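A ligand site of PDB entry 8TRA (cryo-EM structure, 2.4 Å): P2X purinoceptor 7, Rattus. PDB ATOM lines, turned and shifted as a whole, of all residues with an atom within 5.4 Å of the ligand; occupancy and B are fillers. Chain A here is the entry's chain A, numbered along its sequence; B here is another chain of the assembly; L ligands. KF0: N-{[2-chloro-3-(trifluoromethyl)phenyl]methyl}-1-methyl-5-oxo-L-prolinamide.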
ATOM      1  N   ILE A  87      -4.495  12.576  15.386  1.00  0.00           N
ATOM      2  CA  ILE A  87      -4.833  13.908  14.897  1.00  0.00           C
ATOM      3  C   ILE A  87      -3.588  14.487  14.242  1.00  0.00           C
ATOM      4  O   ILE A  87      -2.493  14.468  14.839  1.00  0.00           O
ATOM      5  CB  ILE A  87      -5.331  14.810  16.038  1.00  0.00           C
ATOM      6  CG1 ILE A  87      -5.625  16.213  15.527  1.00  0.00           C
ATOM      7  CG2 ILE A  87      -4.306  14.871  17.175  1.00  0.00           C
ATOM      8  CD1 ILE A  87      -6.727  16.260  14.515  1.00  0.00           C
ATOM      9  N   PHE A  88      -3.733  14.982  13.015  1.00  0.00           N
ATOM     10  CA  PHE A  88      -2.625  15.570  12.268  1.00  0.00           C
ATOM     11  C   PHE A  88      -2.909  17.040  12.018  1.00  0.00           C
ATOM     12  O   PHE A  88      -3.937  17.382  11.421  1.00  0.00           O
ATOM     13  CB  PHE A  88      -2.419  14.838  10.940  1.00  0.00           C
ATOM     14  CG  PHE A  88      -1.908  13.427  11.097  1.00  0.00           C
ATOM     15  CD1 PHE A  88      -2.763  12.410  11.491  1.00  0.00           C
ATOM     16  CD2 PHE A  88      -0.586  13.129  10.844  1.00  0.00           C
ATOM     17  CE1 PHE A  88      -2.299  11.119  11.633  1.00  0.00           C
ATOM     18  CE2 PHE A  88      -0.116  11.836  10.973  1.00  0.00           C
ATOM     19  CZ  PHE A  88      -0.968  10.831  11.374  1.00  0.00           C
ATOM     20  N   THR A  90      -0.702  21.028  11.153  1.00  0.00           N
ATOM     21  CA  THR A  90       0.367  21.507  10.269  1.00  0.00           C
ATOM     22  C   THR A  90       1.731  21.020  10.724  1.00  0.00           C
ATOM     23  O   THR A  90       2.565  20.635   9.900  1.00  0.00           O
ATOM     24  CB  THR A  90       0.336  23.034  10.208  1.00  0.00           C
ATOM     25  OG1 THR A  90       0.255  23.568  11.527  1.00  0.00           O
ATOM     26  CG2 THR A  90      -0.855  23.511   9.392  1.00  0.00           C
ATOM     27  N   ALA A  91       1.976  21.036  12.030  1.00  0.00           N
ATOM     28  CA  ALA A  91       3.266  20.569  12.547  1.00  0.00           C
ATOM     29  C   ALA A  91       3.466  19.070  12.351  1.00  0.00           C
ATOM     30  O   ALA A  91       4.597  18.593  12.484  1.00  0.00           O
ATOM     31  CB  ALA A  91       3.387  20.915  14.033  1.00  0.00           C
ATOM     32  N   ASP A  92       2.398  18.326  12.043  1.00  0.00           N
ATOM     33  CA  ASP A  92       2.488  16.887  11.883  1.00  0.00           C
ATOM     34  C   ASP A  92       2.592  16.438  10.430  1.00  0.00           C
ATOM     35  O   ASP A  92       2.955  15.280  10.184  1.00  0.00           O
ATOM     36  CB  ASP A  92       1.266  16.208  12.528  1.00  0.00           C
ATOM     37  CG  ASP A  92       1.152  16.502  14.005  1.00  0.00           C
ATOM     38  OD1 ASP A  92       2.195  16.506  14.691  1.00  0.00           O
ATOM     39  OD2 ASP A  92       0.019  16.720  14.488  1.00  0.00           O
ATOM     40  N   TYR A  93       2.291  17.318   9.470  1.00  0.00           N
ATOM     41  CA  TYR A  93       2.374  16.941   8.057  1.00  0.00           C
ATOM     42  C   TYR A  93       3.059  18.004   7.207  1.00  0.00           C
ATOM     43  O   TYR A  93       3.065  17.871   5.976  1.00  0.00           O
ATOM     44  CB  TYR A  93       0.976  16.641   7.497  1.00  0.00           C
ATOM     45  CG  TYR A  93       0.051  17.831   7.421  1.00  0.00           C
ATOM     46  CD1 TYR A  93       0.130  18.736   6.366  1.00  0.00           C
ATOM     47  CD2 TYR A  93      -0.923  18.048   8.387  1.00  0.00           C
ATOM     48  CE1 TYR A  93      -0.721  19.829   6.298  1.00  0.00           C
ATOM     49  CE2 TYR A  93      -1.770  19.128   8.324  1.00  0.00           C
ATOM     50  CZ  TYR A  93      -1.664  20.023   7.278  1.00  0.00           C
ATOM     51  OH  TYR A  93      -2.503  21.100   7.203  1.00  0.00           O
ATOM     52  N   THR A  94       3.636  19.038   7.807  1.00  0.00           N
ATOM     53  CA  THR A  94       4.373  20.065   7.081  1.00  0.00           C
ATOM     54  C   THR A  94       5.748  20.250   7.699  1.00  0.00           C
ATOM     55  O   THR A  94       5.906  20.202   8.923  1.00  0.00           O
ATOM     56  CB  THR A  94       3.642  21.421   7.077  1.00  0.00           C
ATOM     57  OG1 THR A  94       3.637  21.970   8.401  1.00  0.00           O
ATOM     58  CG2 THR A  94       2.216  21.263   6.597  1.00  0.00           C
ATOM     59  N   LEU A  95       6.741  20.464   6.849  1.00  0.00           N
ATOM     60  CA  LEU A  95       8.083  20.778   7.295  1.00  0.00           C
ATOM     61  C   LEU A  95       8.223  22.272   7.559  1.00  0.00           C
ATOM     62  O   LEU A  95       7.423  23.083   7.052  1.00  0.00           O
ATOM     63  CB  LEU A  95       9.104  20.338   6.249  1.00  0.00           C
ATOM     64  CG  LEU A  95       9.186  18.826   6.033  1.00  0.00           C
ATOM     65  CD1 LEU A  95       9.792  18.495   4.680  1.00  0.00           C
ATOM     66  CD2 LEU A  95       9.981  18.165   7.152  1.00  0.00           C
ATOM     67  N   PHE A 103       5.788  20.898   1.374  1.00  0.00           N
ATOM     68  CA  PHE A 103       5.396  19.498   1.265  1.00  0.00           C
ATOM     69  C   PHE A 103       4.233  19.227   2.215  1.00  0.00           C
ATOM     70  O   PHE A 103       4.258  19.650   3.376  1.00  0.00           O
ATOM     71  CB  PHE A 103       6.577  18.585   1.613  1.00  0.00           C
ATOM     72  CG  PHE A 103       6.200  17.138   1.782  1.00  0.00           C
ATOM     73  CD1 PHE A 103       6.084  16.301   0.684  1.00  0.00           C
ATOM     74  CD2 PHE A 103       5.951  16.621   3.047  1.00  0.00           C
ATOM     75  CE1 PHE A 103       5.740  14.978   0.847  1.00  0.00           C
ATOM     76  CE2 PHE A 103       5.607  15.297   3.211  1.00  0.00           C
ATOM     77  CZ  PHE A 103       5.501  14.470   2.107  1.00  0.00           C
ATOM     78  N   MET A 105       2.033  15.968   3.662  1.00  0.00           N
ATOM     79  CA  MET A 105       1.967  14.524   3.761  1.00  0.00           C
ATOM     80  C   MET A 105       0.567  14.029   3.423  1.00  0.00           C
ATOM     81  O   MET A 105      -0.435  14.600   3.861  1.00  0.00           O
ATOM     82  CB  MET A 105       2.346  14.065   5.163  1.00  0.00           C
ATOM     83  CG  MET A 105       2.654  12.579   5.266  1.00  0.00           C
ATOM     84  SD  MET A 105       2.011  11.818   6.765  1.00  0.00           S
ATOM     85  CE  MET A 105       3.217  12.368   7.964  1.00  0.00           C
ATOM     86  N   TYR A 108       1.582   7.559   5.007  1.00  0.00           N
ATOM     87  CA  TYR A 108       2.780   7.291   5.794  1.00  0.00           C
ATOM     88  C   TYR A 108       2.814   5.826   6.195  1.00  0.00           C
ATOM     89  O   TYR A 108       1.783   5.193   6.422  1.00  0.00           O
ATOM     90  CB  TYR A 108       2.842   8.175   7.043  1.00  0.00           C
ATOM     91  CG  TYR A 108       1.770   7.879   8.070  1.00  0.00           C
ATOM     92  CD1 TYR A 108       1.990   6.955   9.077  1.00  0.00           C
ATOM     93  CD2 TYR A 108       0.549   8.543   8.048  1.00  0.00           C
ATOM     94  CE1 TYR A 108       1.022   6.685  10.025  1.00  0.00           C
ATOM     95  CE2 TYR A 108      -0.425   8.273   8.985  1.00  0.00           C
ATOM     96  CZ  TYR A 108      -0.184   7.349   9.970  1.00  0.00           C
ATOM     97  OH  TYR A 108      -1.145   7.077  10.906  1.00  0.00           O
ATOM     98  N   LYS A 110       4.730   3.616   9.204  1.00  0.00           N
ATOM     99  CA  LYS A 110       5.371   3.834  10.496  1.00  0.00           C
ATOM    100  C   LYS A 110       6.090   2.569  10.948  1.00  0.00           C
ATOM    101  O   LYS A 110       5.532   1.479  10.888  1.00  0.00           O
ATOM    102  CB  LYS A 110       4.337   4.248  11.548  1.00  0.00           C
ATOM    103  CG  LYS A 110       4.927   4.960  12.753  1.00  0.00           C
ATOM    104  CD  LYS A 110       3.880   5.241  13.807  1.00  0.00           C
ATOM    105  CE  LYS A 110       3.056   6.478  13.466  1.00  0.00           C
ATOM    106  NZ  LYS A 110       1.628   6.324  13.862  1.00  0.00           N
ATOM    107  N   PHE A 293       9.765  10.524   1.366  1.00  0.00           N
ATOM    108  CA  PHE A 293      11.037  10.589   2.066  1.00  0.00           C
ATOM    109  C   PHE A 293      10.879  10.010   3.456  1.00  0.00           C
ATOM    110  O   PHE A 293       9.764   9.891   3.988  1.00  0.00           O
ATOM    111  CB  PHE A 293      11.574  12.027   2.131  1.00  0.00           C
ATOM    112  CG  PHE A 293      10.651  12.998   2.811  1.00  0.00           C
ATOM    113  CD1 PHE A 293      10.697  13.167   4.186  1.00  0.00           C
ATOM    114  CD2 PHE A 293       9.755  13.745   2.070  1.00  0.00           C
ATOM    115  CE1 PHE A 293       9.851  14.064   4.808  1.00  0.00           C
ATOM    116  CE2 PHE A 293       8.909  14.642   2.693  1.00  0.00           C
ATOM    117  CZ  PHE A 293       8.953  14.799   4.060  1.00  0.00           C
ATOM    118  N   TYR A 295      11.538  10.070   7.454  1.00  0.00           N
ATOM    119  CA  TYR A 295      11.674  11.038   8.538  1.00  0.00           C
ATOM    120  C   TYR A 295      11.893  10.267   9.833  1.00  0.00           C
ATOM    121  O   TYR A 295      11.095   9.388  10.174  1.00  0.00           O
ATOM    122  CB  TYR A 295      10.419  11.916   8.605  1.00  0.00           C
ATOM    123  CG  TYR A 295      10.362  12.888   9.764  1.00  0.00           C
ATOM    124  CD1 TYR A 295       9.886  12.493  11.007  1.00  0.00           C
ATOM    125  CD2 TYR A 295      10.756  14.208   9.604  1.00  0.00           C
ATOM    126  CE1 TYR A 295       9.824  13.380  12.058  1.00  0.00           C
ATOM    127  CE2 TYR A 295      10.688  15.103  10.659  1.00  0.00           C
ATOM    128  CZ  TYR A 295      10.221  14.686  11.878  1.00  0.00           C
ATOM    129  OH  TYR A 295      10.159  15.573  12.929  1.00  0.00           O
ATOM    130  N   LYS A 297      12.538  10.040  13.975  1.00  0.00           N
ATOM    131  CA  LYS A 297      12.361  10.630  15.305  1.00  0.00           C
ATOM    132  C   LYS A 297      13.162   9.798  16.288  1.00  0.00           C
ATOM    133  O   LYS A 297      12.851   8.627  16.522  1.00  0.00           O
ATOM    134  CB  LYS A 297      10.880  10.675  15.684  1.00  0.00           C
ATOM    135  CG  LYS A 297      10.031  11.484  14.728  1.00  0.00           C
ATOM    136  CD  LYS A 297       8.655  11.773  15.320  1.00  0.00           C
ATOM    137  CE  LYS A 297       7.817  10.511  15.420  1.00  0.00           C
ATOM    138  NZ  LYS A 297       6.376  10.829  15.614  1.00  0.00           N
ATOM    139  N   ILE A 310       9.412   7.217   9.741  1.00  0.00           N
ATOM    140  CA  ILE A 310       8.196   7.463   8.997  1.00  0.00           C
ATOM    141  C   ILE A 310       8.497   7.551   7.532  1.00  0.00           C
ATOM    142  O   ILE A 310       9.244   8.429   7.115  1.00  0.00           O
ATOM    143  CB  ILE A 310       7.529   8.784   9.399  1.00  0.00           C
ATOM    144  CG1 ILE A 310       7.373   8.871  10.924  1.00  0.00           C
ATOM    145  CG2 ILE A 310       6.185   8.930   8.710  1.00  0.00           C
ATOM    146  CD1 ILE A 310       6.520   7.781  11.519  1.00  0.00           C
ATOM    147  N   ALA A 312       7.144   8.879   4.624  1.00  0.00           N
ATOM    148  CA  ALA A 312       6.051   9.795   4.323  1.00  0.00           C
ATOM    149  C   ALA A 312       5.961   9.985   2.817  1.00  0.00           C
ATOM    150  O   ALA A 312       6.940  10.395   2.173  1.00  0.00           O
ATOM    151  CB  ALA A 312       6.259  11.137   5.018  1.00  0.00           C
ATOM    152  N   GLN B 116      -2.527  13.497  22.326  1.00  0.00           N
ATOM    153  CA  GLN B 116      -3.669  13.448  21.417  1.00  0.00           C
ATOM    154  C   GLN B 116      -4.890  13.010  22.204  1.00  0.00           C
ATOM    155  O   GLN B 116      -5.081  11.824  22.488  1.00  0.00           O
ATOM    156  CB  GLN B 116      -3.390  12.500  20.249  1.00  0.00           C
ATOM    157  CG  GLN B 116      -2.178  12.895  19.424  1.00  0.00           C
ATOM    158  CD  GLN B 116      -1.910  11.928  18.278  1.00  0.00           C
ATOM    159  OE1 GLN B 116      -2.501  12.043  17.210  1.00  0.00           O
ATOM    160  NE2 GLN B 116      -1.014  10.976  18.514  1.00  0.00           N
ATOM    161  N   TRP B 167      -4.007  18.014  19.952  1.00  0.00           N
ATOM    162  CA  TRP B 167      -2.869  17.944  20.850  1.00  0.00           C
ATOM    163  C   TRP B 167      -3.230  18.843  22.015  1.00  0.00           C
ATOM    164  O   TRP B 167      -3.503  20.013  21.811  1.00  0.00           O
ATOM    165  CB  TRP B 167      -1.598  18.373  20.156  1.00  0.00           C
ATOM    166  CG  TRP B 167      -1.081  17.374  19.181  1.00  0.00           C
ATOM    167  CD1 TRP B 167      -1.307  17.350  17.838  1.00  0.00           C
ATOM    168  CD2 TRP B 167      -0.239  16.260  19.467  1.00  0.00           C
ATOM    169  NE1 TRP B 167      -0.661  16.286  17.271  1.00  0.00           N
ATOM    170  CE2 TRP B 167       0.004  15.599  18.243  1.00  0.00           C
ATOM    171  CE3 TRP B 167       0.334  15.743  20.635  1.00  0.00           C
ATOM    172  CZ2 TRP B 167       0.792  14.454  18.156  1.00  0.00           C
ATOM    173  CZ3 TRP B 167       1.117  14.611  20.543  1.00  0.00           C
ATOM    174  CH2 TRP B 167       1.344  13.977  19.322  1.00  0.00           C
ATOM    175  N   TYR B 298       8.935  15.513  19.332  1.00  0.00           N
ATOM    176  CA  TYR B 298       8.251  14.307  19.795  1.00  0.00           C
ATOM    177  C   TYR B 298       9.168  13.511  20.720  1.00  0.00           C
ATOM    178  O   TYR B 298      10.343  13.316  20.417  1.00  0.00           O
ATOM    179  CB  TYR B 298       7.818  13.446  18.613  1.00  0.00           C
ATOM    180  CG  TYR B 298       7.025  14.183  17.563  1.00  0.00           C
ATOM    181  CD1 TYR B 298       7.657  14.828  16.519  1.00  0.00           C
ATOM    182  CD2 TYR B 298       5.633  14.226  17.624  1.00  0.00           C
ATOM    183  CE1 TYR B 298       6.937  15.497  15.553  1.00  0.00           C
ATOM    184  CE2 TYR B 298       4.900  14.898  16.659  1.00  0.00           C
ATOM    185  CZ  TYR B 298       5.559  15.532  15.623  1.00  0.00           C
ATOM    186  OH  TYR B 298       4.833  16.204  14.670  1.00  0.00           O
ATOM    187  N   GLU B 305       3.359   8.691  23.759  1.00  0.00           N
ATOM    188  CA  GLU B 305       3.972   9.625  22.814  1.00  0.00           C
ATOM    189  C   GLU B 305       3.481  11.033  23.123  1.00  0.00           C
ATOM    190  O   GLU B 305       2.270  11.292  23.086  1.00  0.00           O
ATOM    191  CB  GLU B 305       3.633   9.233  21.382  1.00  0.00           C
ATOM    192  CG  GLU B 305       4.249   7.912  20.928  1.00  0.00           C
ATOM    193  CD  GLU B 305       3.825   7.528  19.514  1.00  0.00           C
ATOM    194  OE1 GLU B 305       2.913   8.181  18.961  1.00  0.00           O
ATOM    195  OE2 GLU B 305       4.414   6.571  18.969  1.00  0.00           O
HETATM  196  C10 KF0 L   1       2.074  12.735  13.859  1.00  0.00           C
HETATM  197  C13 KF0 L   1       4.339  12.453  12.668  1.00  0.00           C
HETATM  198  C15 KF0 L   1       6.237  14.152  12.182  1.00  0.00           C
HETATM  199  C17 KF0 L   1       6.463  14.885   9.678  1.00  0.00           C
HETATM  200  C20 KF0 L   1       6.680  17.635  10.340  1.00  0.00           C
HETATM  201  C21 KF0 L   1       6.715  17.235   8.955  1.00  0.00           C
HETATM  202  C22 KF0 L   1       6.639  15.385   7.102  1.00  0.00           C
HETATM  203  C09 KF0 L   1       2.813  12.132  12.628  1.00  0.00           C
HETATM  204  C11 KF0 L   1       2.000  11.576  14.858  1.00  0.00           C
HETATM  205  C12 KF0 L   1       2.034  10.335  13.981  1.00  0.00           C
HETATM  206  C14 KF0 L   1       2.695   9.746  11.527  1.00  0.00           C
HETATM  207  C16 KF0 L   1       6.432  15.241  11.049  1.00  0.00           C
HETATM  208  C18 KF0 L   1       6.532  16.642  11.383  1.00  0.00           C
HETATM  209  C19 KF0 L   1       6.596  15.839   8.634  1.00  0.00           C
HETATM  210  F02 KF0 L   1       6.924  16.366   6.183  1.00  0.00           F
HETATM  211  F03 KF0 L   1       5.472  14.835   6.606  1.00  0.00           F
HETATM  212  F04 KF0 L   1       7.566  14.405   6.766  1.00  0.00           F
HETATM  213  N07 KF0 L   1       2.512  10.672  12.669  1.00  0.00           N
HETATM  214  N08 KF0 L   1       4.831  13.706  12.223  1.00  0.00           N
HETATM  215  O05 KF0 L   1       1.691   9.212  14.367  1.00  0.00           O
HETATM  216  O06 KF0 L   1       5.124  11.611  13.108  1.00  0.00           O
HETATM  217 CL01 KF0 L   1       6.316  13.090   9.248  1.00  0.00          CL
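The side-chain amino group of Lys 297 sits at hydrogen-bond distance from an oxygen (O06) of the ligand (2.9 Å).
NZ of Lys 110 lies within hydrogen-bond range of O05 of the ligand, 2.9 Å away.
A nitrogen (N08) of the ligand sits at hydrogen-bond distance from the backbone carbonyl oxygen of Asp 92 (3.2 Å).
The side-chain hydroxyl (OH) of Tyr 298 of chain B is in hydrogen-bond range of a nitrogen (N08) of the ligand.
The backbone carbonyl oxygen (O) of Ala 91 lies within hydrogen-bond range of the side-chain hydroxyl (OH) of Tyr 298 of chain B (3.2 Å).
The backbone carbonyl oxygen (O) of Phe 293 is in hydrogen-bond range of the backbone NH (N) of Ala 312, 2.9 Å away.
The side-chain carboxylate (OD1) of Asp 92 lies within hydrogen-bond range of the side-chain hydroxyl (OH) of Tyr 298 of chain B (2.7 Å).
OD2 of Asp 92 is in hydrogen-bond range of NE1 of Trp 167 of chain B, 2.9 Å away.
N of Met 105 lies within hydrogen-bond range of O of Tyr 93, 3.2 Å away.
The backbone carbonyl oxygen (O) of Tyr 295 is in hydrogen-bond range of the backbone NH (N) of Ile 310, at 2.8 Å.
Phe 88 touches the ligand (CE2 to N07, 3.3 Å).
Ala 91 touches the ligand (O to C18, 3.0 Å).
Tyr 93 touches the ligand.
O of Thr 94 touches C20 of the ligand (3.0 Å).
Leu 95 touches the ligand.
CD2 of Phe 103 touches F02 of the ligand, 3.3 Å away.
Met 105 touches the ligand.
Tyr 108 touches the ligand.
Phe 293 touches the ligand (CE1 to F04, 3.0 Å).
CE1 of Tyr 295 touches C15 of the ligand, 3.7 Å away.
Ala 312 touches the ligand (CB to F04, 3.9 Å).
Hydrophobic or aromatic side chains that line the ligand: Phe 88, Leu 95, Phe 103, Met 105, Tyr 108, Phe 293, Tyr 295, Ala 312 and Tyr 298 of chain B.
Of the 21 residues printed, 15 come within 4 Å of the ligand.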
